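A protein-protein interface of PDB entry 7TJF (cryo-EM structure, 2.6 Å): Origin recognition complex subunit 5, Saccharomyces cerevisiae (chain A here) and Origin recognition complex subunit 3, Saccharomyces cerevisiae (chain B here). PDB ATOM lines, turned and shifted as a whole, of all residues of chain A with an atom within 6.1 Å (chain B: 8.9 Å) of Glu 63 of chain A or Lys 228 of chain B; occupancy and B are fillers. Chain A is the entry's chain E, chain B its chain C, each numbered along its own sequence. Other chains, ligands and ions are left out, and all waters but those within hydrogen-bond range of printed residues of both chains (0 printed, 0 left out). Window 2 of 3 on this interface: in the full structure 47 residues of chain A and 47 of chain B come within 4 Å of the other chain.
Printed residues of chain B within 4 Å of Glu 63 of chain A: Lys 228 (3.3 Å). Of chain A, only Glu 63 (3.3 Å) and Glu 66 (2.5 Å) come within 4 Å of Lys 228 of chain B. No residue of chain B comes within 4 Å of Pro 64 of chain A. Of the printed residues of chain A, Leu 222 of chain B touches Val 65. Printed residues of chain A within 4 Å of Leu 185 of chain B: Glu 66. Of the printed residues of chain A, Asp 184 of chain B touches Glu 66 and Leu 67. Phe 227 of chain B touches none of the printed residues of chain A. Lys 224 of chain B touches none of the printed residues of chain A. The nearest printed residue of chain A that does not touch Lys 228 of chain B is Val 65 of chain A (6.6 Å).
O of Glu 66 of chain A lies within hydrogen-bond range of N of Leu 185 of chain B (3.3 Å). The side-chain amino group (NZ) of Lys 228 of chain B is in salt-bridge range of the side-chain carboxylate (OE2) of Glu 63 of chain A (3.7 Å). The side-chain amino group (NZ) of Lys 228 of chain B is in salt-bridge range of the side-chain carboxylate (OE2) of Glu 66 of chain A (2.5 Å). The side-chain carboxylate of Glu 66 of chain A is in hydrogen-bond range of the side-chain hydroxyl of Tyr 229 of chain B, 2.8 Å away.
Val 65 of chain A touches Leu 222 of chain B. Ser 225 of chain B touches Val 65 of chain A. O of Glu 66 of chain A touches CB of Asp 184 of chain B, at 3.9 Å. Ser 225 of chain B touches Glu 66 of chain A. CD1 of Leu 67 of chain A touches CG of Asp 184 of chain B, 3.7 Å away.
The side-chain carboxylate of Asp 184 of chain B lies within hydrogen-bond range of the backbone NH of Ser 186 of chain B. O of Leu 222 of chain B sits at hydrogen-bond distance from OG of Ser 225 of chain B, at 3.1 Å. The backbone carbonyl oxygen of Ser 225 of chain B is in hydrogen-bond range of the side-chain amino group of Lys 228 of chain B (2.9 Å). OH of Tyr 229 of chain B sits close to NZ of Lys 228 of chain B.
Hydrophobic or aromatic side chains of chain B within 4 Å of the printed part of chain A: Leu 185, Leu 222 and Tyr 229. Hydrophobic or aromatic side chains of chain A within 4 Å of the printed part of chain B: Val 65 and Leu 67. Among the printed residues, Asp or Glu carboxylates within 4 Å of a Lys or Arg side-chain nitrogen of the other chain: Glu 63 of chain A with Lys 228 of chain B (3.7 Å) and Glu 66 of chain A with Lys 228 of chain B (2.5 Å).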
ATOM      1  N   TRP A  61      21.186   1.251  38.387  1.00  0.00           N
ATOM      2  CA  TRP A  61      20.813   1.639  37.032  1.00  0.00           C
ATOM      3  C   TRP A  61      21.304   0.593  36.038  1.00  0.00           C
ATOM      4  O   TRP A  61      22.504   0.310  35.969  1.00  0.00           O
ATOM      5  CB  TRP A  61      21.382   3.013  36.681  1.00  0.00           C
ATOM      6  CG  TRP A  61      20.718   4.139  37.406  1.00  0.00           C
ATOM      7  CD1 TRP A  61      20.998   4.579  38.663  1.00  0.00           C
ATOM      8  CD2 TRP A  61      19.652   4.964  36.920  1.00  0.00           C
ATOM      9  NE1 TRP A  61      20.179   5.631  38.991  1.00  0.00           N
ATOM     10  CE2 TRP A  61      19.343   5.888  37.936  1.00  0.00           C
ATOM     11  CE3 TRP A  61      18.932   5.011  35.723  1.00  0.00           C
ATOM     12  CZ2 TRP A  61      18.340   6.847  37.795  1.00  0.00           C
ATOM     13  CZ3 TRP A  61      17.939   5.967  35.583  1.00  0.00           C
ATOM     14  CH2 TRP A  61      17.654   6.872  36.613  1.00  0.00           C
ATOM     15  N   LEU A  62      20.375   0.029  35.272  1.00  0.00           N
ATOM     16  CA  LEU A  62      20.690  -0.904  34.199  1.00  0.00           C
ATOM     17  C   LEU A  62      20.053  -0.406  32.916  1.00  0.00           C
ATOM     18  O   LEU A  62      18.874  -0.040  32.906  1.00  0.00           O
ATOM     19  CB  LEU A  62      20.189  -2.320  34.503  1.00  0.00           C
ATOM     20  CG  LEU A  62      21.114  -3.272  35.253  1.00  0.00           C
ATOM     21  CD1 LEU A  62      21.128  -2.930  36.717  1.00  0.00           C
ATOM     22  CD2 LEU A  62      20.685  -4.712  35.041  1.00  0.00           C
ATOM     23  N   GLU A  63      20.826  -0.396  31.841  1.00  0.00           N
ATOM     24  CA  GLU A  63      20.292  -0.066  30.529  1.00  0.00           C
ATOM     25  C   GLU A  63      20.269  -1.328  29.685  1.00  0.00           C
ATOM     26  O   GLU A  63      21.328  -1.764  29.212  1.00  0.00           O
ATOM     27  CB  GLU A  63      21.126   1.022  29.856  1.00  0.00           C
ATOM     28  CG  GLU A  63      20.800   2.421  30.350  1.00  0.00           C
ATOM     29  CD  GLU A  63      21.715   2.874  31.470  1.00  0.00           C
ATOM     30  OE1 GLU A  63      21.533   2.415  32.618  1.00  0.00           O
ATOM     31  OE2 GLU A  63      22.613   3.697  31.204  1.00  0.00           O
ATOM     32  N   PRO A  64      19.106  -1.939  29.457  1.00  0.00           N
ATOM     33  CA  PRO A  64      19.058  -3.226  28.753  1.00  0.00           C
ATOM     34  C   PRO A  64      19.296  -3.151  27.254  1.00  0.00           C
ATOM     35  O   PRO A  64      19.246  -4.190  26.593  1.00  0.00           O
ATOM     36  CB  PRO A  64      17.628  -3.719  29.038  1.00  0.00           C
ATOM     37  CG  PRO A  64      17.157  -2.929  30.206  1.00  0.00           C
ATOM     38  CD  PRO A  64      17.816  -1.606  30.081  1.00  0.00           C
ATOM     39  N   VAL A  65      19.589  -1.987  26.686  1.00  0.00           N
ATOM     40  CA  VAL A  65      19.974  -1.961  25.285  1.00  0.00           C
ATOM     41  C   VAL A  65      21.419  -2.430  25.127  1.00  0.00           C
ATOM     42  O   VAL A  65      21.783  -2.964  24.078  1.00  0.00           O
ATOM     43  CB  VAL A  65      19.731  -0.563  24.672  1.00  0.00           C
ATOM     44  CG1 VAL A  65      20.768   0.462  25.123  1.00  0.00           C
ATOM     45  CG2 VAL A  65      19.652  -0.639  23.151  1.00  0.00           C
ATOM     46  N   GLU A  66      22.233  -2.298  26.180  1.00  0.00           N
ATOM     47  CA  GLU A  66      23.607  -2.778  26.163  1.00  0.00           C
ATOM     48  C   GLU A  66      23.707  -4.286  26.369  1.00  0.00           C
ATOM     49  O   GLU A  66      24.744  -4.873  26.044  1.00  0.00           O
ATOM     50  CB  GLU A  66      24.416  -2.046  27.235  1.00  0.00           C
ATOM     51  CG  GLU A  66      24.375  -0.533  27.106  1.00  0.00           C
ATOM     52  CD  GLU A  66      25.268   0.172  28.107  1.00  0.00           C
ATOM     53  OE1 GLU A  66      26.421  -0.272  28.301  1.00  0.00           O
ATOM     54  OE2 GLU A  66      24.820   1.178  28.697  1.00  0.00           O
ATOM     55  N   LEU A  67      22.668  -4.923  26.914  1.00  0.00           N
ATOM     56  CA  LEU A  67      22.730  -6.345  27.238  1.00  0.00           C
ATOM     57  C   LEU A  67      22.131  -7.253  26.170  1.00  0.00           C
ATOM     58  O   LEU A  67      22.448  -8.450  26.160  1.00  0.00           O
ATOM     59  CB  LEU A  67      22.044  -6.625  28.581  1.00  0.00           C
ATOM     60  CG  LEU A  67      22.696  -6.132  29.883  1.00  0.00           C
ATOM     61  CD1 LEU A  67      24.222  -6.217  29.823  1.00  0.00           C
ATOM     62  CD2 LEU A  67      22.247  -4.745  30.279  1.00  0.00           C
ATOM     63  N   ILE A 131      16.400  -0.199  38.329  1.00  0.00           N
ATOM     64  CA  ILE A 131      15.862   0.611  37.244  1.00  0.00           C
ATOM     65  C   ILE A 131      16.260  -0.035  35.924  1.00  0.00           C
ATOM     66  O   ILE A 131      17.434  -0.042  35.551  1.00  0.00           O
ATOM     67  CB  ILE A 131      16.350   2.061  37.332  1.00  0.00           C
ATOM     68  CG1 ILE A 131      15.871   2.688  38.640  1.00  0.00           C
ATOM     69  CG2 ILE A 131      15.852   2.860  36.146  1.00  0.00           C
ATOM     70  CD1 ILE A 131      16.696   3.840  39.092  1.00  0.00           C
ATOM     71  N   LEU A 132      15.274  -0.579  35.217  1.00  0.00           N
ATOM     72  CA  LEU A 132      15.493  -1.200  33.915  1.00  0.00           C
ATOM     73  C   LEU A 132      15.116  -0.160  32.863  1.00  0.00           C
ATOM     74  O   LEU A 132      14.040  -0.188  32.265  1.00  0.00           O
ATOM     75  CB  LEU A 132      14.694  -2.496  33.787  1.00  0.00           C
ATOM     76  CG  LEU A 132      15.358  -3.799  34.270  1.00  0.00           C
ATOM     77  CD1 LEU A 132      15.585  -3.840  35.775  1.00  0.00           C
ATOM     78  CD2 LEU A 132      14.547  -5.006  33.847  1.00  0.00           C
ATOM     79  N   ASP A 133      16.034   0.783  32.657  1.00  0.00           N
ATOM     80  CA  ASP A 133      15.825   1.939  31.796  1.00  0.00           C
ATOM     81  C   ASP A 133      15.864   1.531  30.328  1.00  0.00           C
ATOM     82  O   ASP A 133      16.932   1.519  29.712  1.00  0.00           O
ATOM     83  CB  ASP A 133      16.889   3.000  32.100  1.00  0.00           C
ATOM     84  CG  ASP A 133      16.513   4.392  31.603  1.00  0.00           C
ATOM     85  OD1 ASP A 133      15.506   4.544  30.890  1.00  0.00           O
ATOM     86  OD2 ASP A 133      17.245   5.345  31.934  1.00  0.00           O
ATOM     87  N   GLY A 134      14.700   1.250  29.746  1.00  0.00           N
ATOM     88  CA  GLY A 134      14.641   0.747  28.390  1.00  0.00           C
ATOM     89  C   GLY A 134      14.479  -0.755  28.287  1.00  0.00           C
ATOM     90  O   GLY A 134      15.281  -1.419  27.624  1.00  0.00           O
ATOM     91  N   ARG B 100      32.402  13.367  22.166  1.00  0.00           N
ATOM     92  CA  ARG B 100      31.672  12.132  22.422  1.00  0.00           C
ATOM     93  C   ARG B 100      30.882  11.698  21.194  1.00  0.00           C
ATOM     94  O   ARG B 100      29.661  11.837  21.150  1.00  0.00           O
ATOM     95  CB  ARG B 100      30.737  12.302  23.619  1.00  0.00           C
ATOM     96  CG  ARG B 100      31.446  12.645  24.920  1.00  0.00           C
ATOM     97  CD  ARG B 100      32.265  11.471  25.427  1.00  0.00           C
ATOM     98  NE  ARG B 100      33.216  11.866  26.459  1.00  0.00           N
ATOM     99  CZ  ARG B 100      34.386  11.276  26.666  1.00  0.00           C
ATOM    100  NH1 ARG B 100      34.781  10.249  25.930  1.00  0.00           N
ATOM    101  NH2 ARG B 100      35.176  11.722  27.638  1.00  0.00           N
ATOM    102  N   CYS B 101      31.589  11.167  20.201  1.00  0.00           N
ATOM    103  CA  CYS B 101      30.974  10.739  18.952  1.00  0.00           C
ATOM    104  C   CYS B 101      31.877   9.706  18.292  1.00  0.00           C
ATOM    105  O   CYS B 101      33.019   9.497  18.704  1.00  0.00           O
ATOM    106  CB  CYS B 101      30.729  11.928  18.019  1.00  0.00           C
ATOM    107  SG  CYS B 101      32.195  12.928  17.717  1.00  0.00           S
ATOM    108  N   ASP B 184      29.045  -8.869  26.174  1.00  0.00           N
ATOM    109  CA  ASP B 184      28.082  -7.805  25.954  1.00  0.00           C
ATOM    110  C   ASP B 184      28.779  -6.479  26.239  1.00  0.00           C
ATOM    111  O   ASP B 184      29.970  -6.442  26.558  1.00  0.00           O
ATOM    112  CB  ASP B 184      26.797  -8.091  26.763  1.00  0.00           C
ATOM    113  CG  ASP B 184      26.989  -8.040  28.291  1.00  0.00           C
ATOM    114  OD1 ASP B 184      27.637  -7.147  28.863  1.00  0.00           O
ATOM    115  OD2 ASP B 184      26.505  -8.974  28.948  1.00  0.00           O
ATOM    116  N   LEU B 185      28.016  -5.389  26.166  1.00  0.00           N
ATOM    117  CA  LEU B 185      28.605  -4.059  26.265  1.00  0.00           C
ATOM    118  C   LEU B 185      29.015  -3.674  27.684  1.00  0.00           C
ATOM    119  O   LEU B 185      29.644  -2.627  27.858  1.00  0.00           O
ATOM    120  CB  LEU B 185      27.640  -3.018  25.693  1.00  0.00           C
ATOM    121  CG  LEU B 185      28.284  -1.849  24.943  1.00  0.00           C
ATOM    122  CD1 LEU B 185      29.066  -2.346  23.732  1.00  0.00           C
ATOM    123  CD2 LEU B 185      27.238  -0.823  24.538  1.00  0.00           C
ATOM    124  N   SER B 186      28.690  -4.480  28.701  1.00  0.00           N
ATOM    125  CA  SER B 186      29.231  -4.209  30.031  1.00  0.00           C
ATOM    126  C   SER B 186      30.712  -4.554  30.132  1.00  0.00           C
ATOM    127  O   SER B 186      31.365  -4.133  31.091  1.00  0.00           O
ATOM    128  CB  SER B 186      28.447  -4.955  31.113  1.00  0.00           C
ATOM    129  OG  SER B 186      28.393  -6.344  30.855  1.00  0.00           O
ATOM    130  N   VAL B 188      32.697  -3.326  27.920  1.00  0.00           N
ATOM    131  CA  VAL B 188      33.227  -2.017  27.548  1.00  0.00           C
ATOM    132  C   VAL B 188      33.262  -1.083  28.754  1.00  0.00           C
ATOM    133  O   VAL B 188      34.263  -0.397  28.993  1.00  0.00           O
ATOM    134  CB  VAL B 188      32.398  -1.434  26.384  1.00  0.00           C
ATOM    135  CG1 VAL B 188      32.715   0.029  26.148  1.00  0.00           C
ATOM    136  CG2 VAL B 188      32.638  -2.231  25.128  1.00  0.00           C
ATOM    137  N   GLU B 189      32.186  -1.061  29.548  1.00  0.00           N
ATOM    138  CA  GLU B 189      32.136  -0.162  30.698  1.00  0.00           C
ATOM    139  C   GLU B 189      33.021  -0.622  31.844  1.00  0.00           C
ATOM    140  O   GLU B 189      33.393   0.198  32.689  1.00  0.00           O
ATOM    141  CB  GLU B 189      30.702  -0.004  31.201  1.00  0.00           C
ATOM    142  CG  GLU B 189      30.119  -1.184  31.951  1.00  0.00           C
ATOM    143  CD  GLU B 189      28.865  -0.821  32.721  1.00  0.00           C
ATOM    144  OE1 GLU B 189      28.972  -0.064  33.708  1.00  0.00           O
ATOM    145  OE2 GLU B 189      27.773  -1.295  32.341  1.00  0.00           O
ATOM    146  N   LEU B 222      23.352   0.735  18.951  1.00  0.00           N
ATOM    147  CA  LEU B 222      23.884   0.035  20.120  1.00  0.00           C
ATOM    148  C   LEU B 222      25.232   0.607  20.553  1.00  0.00           C
ATOM    149  O   LEU B 222      25.460   0.831  21.748  1.00  0.00           O
ATOM    150  CB  LEU B 222      24.012  -1.461  19.815  1.00  0.00           C
ATOM    151  CG  LEU B 222      24.699  -2.467  20.758  1.00  0.00           C
ATOM    152  CD1 LEU B 222      24.358  -2.275  22.228  1.00  0.00           C
ATOM    153  CD2 LEU B 222      24.392  -3.894  20.337  1.00  0.00           C
ATOM    154  N   LEU B 223      26.133   0.855  19.600  1.00  0.00           N
ATOM    155  CA  LEU B 223      27.454   1.379  19.938  1.00  0.00           C
ATOM    156  C   LEU B 223      27.404   2.826  20.415  1.00  0.00           C
ATOM    157  O   LEU B 223      28.365   3.289  21.037  1.00  0.00           O
ATOM    158  CB  LEU B 223      28.396   1.259  18.739  1.00  0.00           C
ATOM    159  CG  LEU B 223      28.839  -0.148  18.341  1.00  0.00           C
ATOM    160  CD1 LEU B 223      29.773  -0.097  17.139  1.00  0.00           C
ATOM    161  CD2 LEU B 223      29.487  -0.868  19.516  1.00  0.00           C
ATOM    162  N   LYS B 224      26.309   3.541  20.128  1.00  0.00           N
ATOM    163  CA  LYS B 224      26.100   4.880  20.681  1.00  0.00           C
ATOM    164  C   LYS B 224      26.038   4.882  22.210  1.00  0.00           C
ATOM    165  O   LYS B 224      26.352   5.899  22.838  1.00  0.00           O
ATOM    166  CB  LYS B 224      24.811   5.482  20.124  1.00  0.00           C
ATOM    167  CG  LYS B 224      24.756   6.997  20.132  1.00  0.00           C
ATOM    168  CD  LYS B 224      23.315   7.483  20.204  1.00  0.00           C
ATOM    169  CE  LYS B 224      22.701   7.643  18.831  1.00  0.00           C
ATOM    170  NZ  LYS B 224      21.723   8.759  18.783  1.00  0.00           N
ATOM    171  N   SER B 225      25.637   3.759  22.822  1.00  0.00           N
ATOM    172  CA  SER B 225      25.523   3.667  24.276  1.00  0.00           C
ATOM    173  C   SER B 225      26.867   3.737  24.991  1.00  0.00           C
ATOM    174  O   SER B 225      26.896   3.994  26.198  1.00  0.00           O
ATOM    175  CB  SER B 225      24.810   2.371  24.665  1.00  0.00           C
ATOM    176  OG  SER B 225      23.676   2.138  23.851  1.00  0.00           O
ATOM    177  N   ALA B 226      27.975   3.522  24.286  1.00  0.00           N
ATOM    178  CA  ALA B 226      29.297   3.589  24.893  1.00  0.00           C
ATOM    179  C   ALA B 226      29.838   5.010  24.999  1.00  0.00           C
ATOM    180  O   ALA B 226      30.933   5.193  25.543  1.00  0.00           O
ATOM    181  CB  ALA B 226      30.278   2.720  24.104  1.00  0.00           C
ATOM    182  N   PHE B 227      29.110   6.014  24.501  1.00  0.00           N
ATOM    183  CA  PHE B 227      29.585   7.393  24.563  1.00  0.00           C
ATOM    184  C   PHE B 227      29.529   7.975  25.969  1.00  0.00           C
ATOM    185  O   PHE B 227      30.194   8.981  26.234  1.00  0.00           O
ATOM    186  CB  PHE B 227      28.778   8.282  23.617  1.00  0.00           C
ATOM    187  CG  PHE B 227      29.019   7.997  22.164  1.00  0.00           C
ATOM    188  CD1 PHE B 227      30.234   7.483  21.735  1.00  0.00           C
ATOM    189  CD2 PHE B 227      28.031   8.253  21.225  1.00  0.00           C
ATOM    190  CE1 PHE B 227      30.455   7.223  20.398  1.00  0.00           C
ATOM    191  CE2 PHE B 227      28.248   7.997  19.886  1.00  0.00           C
ATOM    192  CZ  PHE B 227      29.460   7.479  19.475  1.00  0.00           C
ATOM    193  N   LYS B 228      28.760   7.378  26.874  1.00  0.00           N
ATOM    194  CA  LYS B 228      28.673   7.893  28.233  1.00  0.00           C
ATOM    195  C   LYS B 228      29.821   7.432  29.118  1.00  0.00           C
ATOM    196  O   LYS B 228      29.890   7.842  30.280  1.00  0.00           O
ATOM    197  CB  LYS B 228      27.339   7.495  28.863  1.00  0.00           C
ATOM    198  CG  LYS B 228      27.194   6.014  29.141  1.00  0.00           C
ATOM    199  CD  LYS B 228      25.897   5.741  29.878  1.00  0.00           C
ATOM    200  CE  LYS B 228      25.625   4.261  29.981  1.00  0.00           C
ATOM    201  NZ  LYS B 228      25.357   3.642  28.652  1.00  0.00           N
ATOM    202  N   TYR B 229      30.717   6.597  28.604  1.00  0.00           N
ATOM    203  CA  TYR B 229      31.892   6.159  29.340  1.00  0.00           C
ATOM    204  C   TYR B 229      33.083   6.994  28.892  1.00  0.00           C
ATOM    205  O   TYR B 229      33.327   7.141  27.690  1.00  0.00           O
ATOM    206  CB  TYR B 229      32.141   4.669  29.114  1.00  0.00           C
ATOM    207  CG  TYR B 229      30.907   3.834  29.377  1.00  0.00           C
ATOM    208  CD1 TYR B 229      30.221   3.936  30.584  1.00  0.00           C
ATOM    209  CD2 TYR B 229      30.409   2.967  28.411  1.00  0.00           C
ATOM    210  CE1 TYR B 229      29.083   3.187  30.827  1.00  0.00           C
ATOM    211  CE2 TYR B 229      29.272   2.211  28.645  1.00  0.00           C
ATOM    212  CZ  TYR B 229      28.608   2.332  29.850  1.00  0.00           C
ATOM    213  OH  TYR B 229      27.487   1.575  30.090  1.00  0.00           O
ATOM    214  N   ASP B 230      33.810   7.550  29.856  1.00  0.00           N
ATOM    215  CA  ASP B 230      34.845   8.532  29.568  1.00  0.00           C
ATOM    216  C   ASP B 230      36.157   7.905  29.121  1.00  0.00           C
ATOM    217  O   ASP B 230      37.067   8.635  28.715  1.00  0.00           O
ATOM    218  CB  ASP B 230      35.089   9.406  30.800  1.00  0.00           C
ATOM    219  CG  ASP B 230      33.804   9.795  31.500  1.00  0.00           C
ATOM    220  OD1 ASP B 230      32.762   9.894  30.820  1.00  0.00           O
ATOM    221  OD2 ASP B 230      33.835  10.001  32.732  1.00  0.00           O
ATOM    222  N   HIS B 231      36.277   6.582  29.179  1.00  0.00           N
ATOM    223  CA  HIS B 231      37.503   5.886  28.818  1.00  0.00           C
ATOM    224  C   HIS B 231      37.398   5.179  27.475  1.00  0.00           C
ATOM    225  O   HIS B 231      38.263   4.359  27.149  1.00  0.00           O
ATOM    226  CB  HIS B 231      37.872   4.885  29.913  1.00  0.00           C
ATOM    227  CG  HIS B 231      36.775   3.923  30.249  1.00  0.00           C
ATOM    228  ND1 HIS B 231      35.761   4.229  31.129  1.00  0.00           N
ATOM    229  CD2 HIS B 231      36.535   2.661  29.824  1.00  0.00           C
ATOM    230  CE1 HIS B 231      34.941   3.200  31.230  1.00  0.00           C
ATOM    231  NE2 HIS B 231      35.388   2.234  30.448  1.00  0.00           N
ATOM    232  N   VAL B 232      36.357   5.464  26.694  1.00  0.00           N
ATOM    233  CA  VAL B 232      36.079   4.768  25.442  1.00  0.00           C
ATOM    234  C   VAL B 232      35.988   5.788  24.314  1.00  0.00           C
ATOM    235  O   VAL B 232      35.261   6.781  24.428  1.00  0.00           O
ATOM    236  CB  VAL B 232      34.774   3.951  25.523  1.00  0.00           C
ATOM    237  CG1 VAL B 232      34.585   3.116  24.268  1.00  0.00           C
ATOM    238  CG2 VAL B 232      34.745   3.069  26.764  1.00  0.00           C
ATOM    239  N   ILE B 234      35.396   5.381  19.930  1.00  0.00           N
ATOM    240  CA  ILE B 234      35.041   4.410  18.901  1.00  0.00           C
ATOM    241  C   ILE B 234      35.273   5.031  17.528  1.00  0.00           C
ATOM    242  O   ILE B 234      34.804   6.142  17.249  1.00  0.00           O
ATOM    243  CB  ILE B 234      33.582   3.927  19.044  1.00  0.00           C
ATOM    244  CG1 ILE B 234      33.341   3.316  20.426  1.00  0.00           C
ATOM    245  CG2 ILE B 234      33.247   2.888  17.979  1.00  0.00           C
ATOM    246  CD1 ILE B 234      31.900   2.969  20.694  1.00  0.00           C
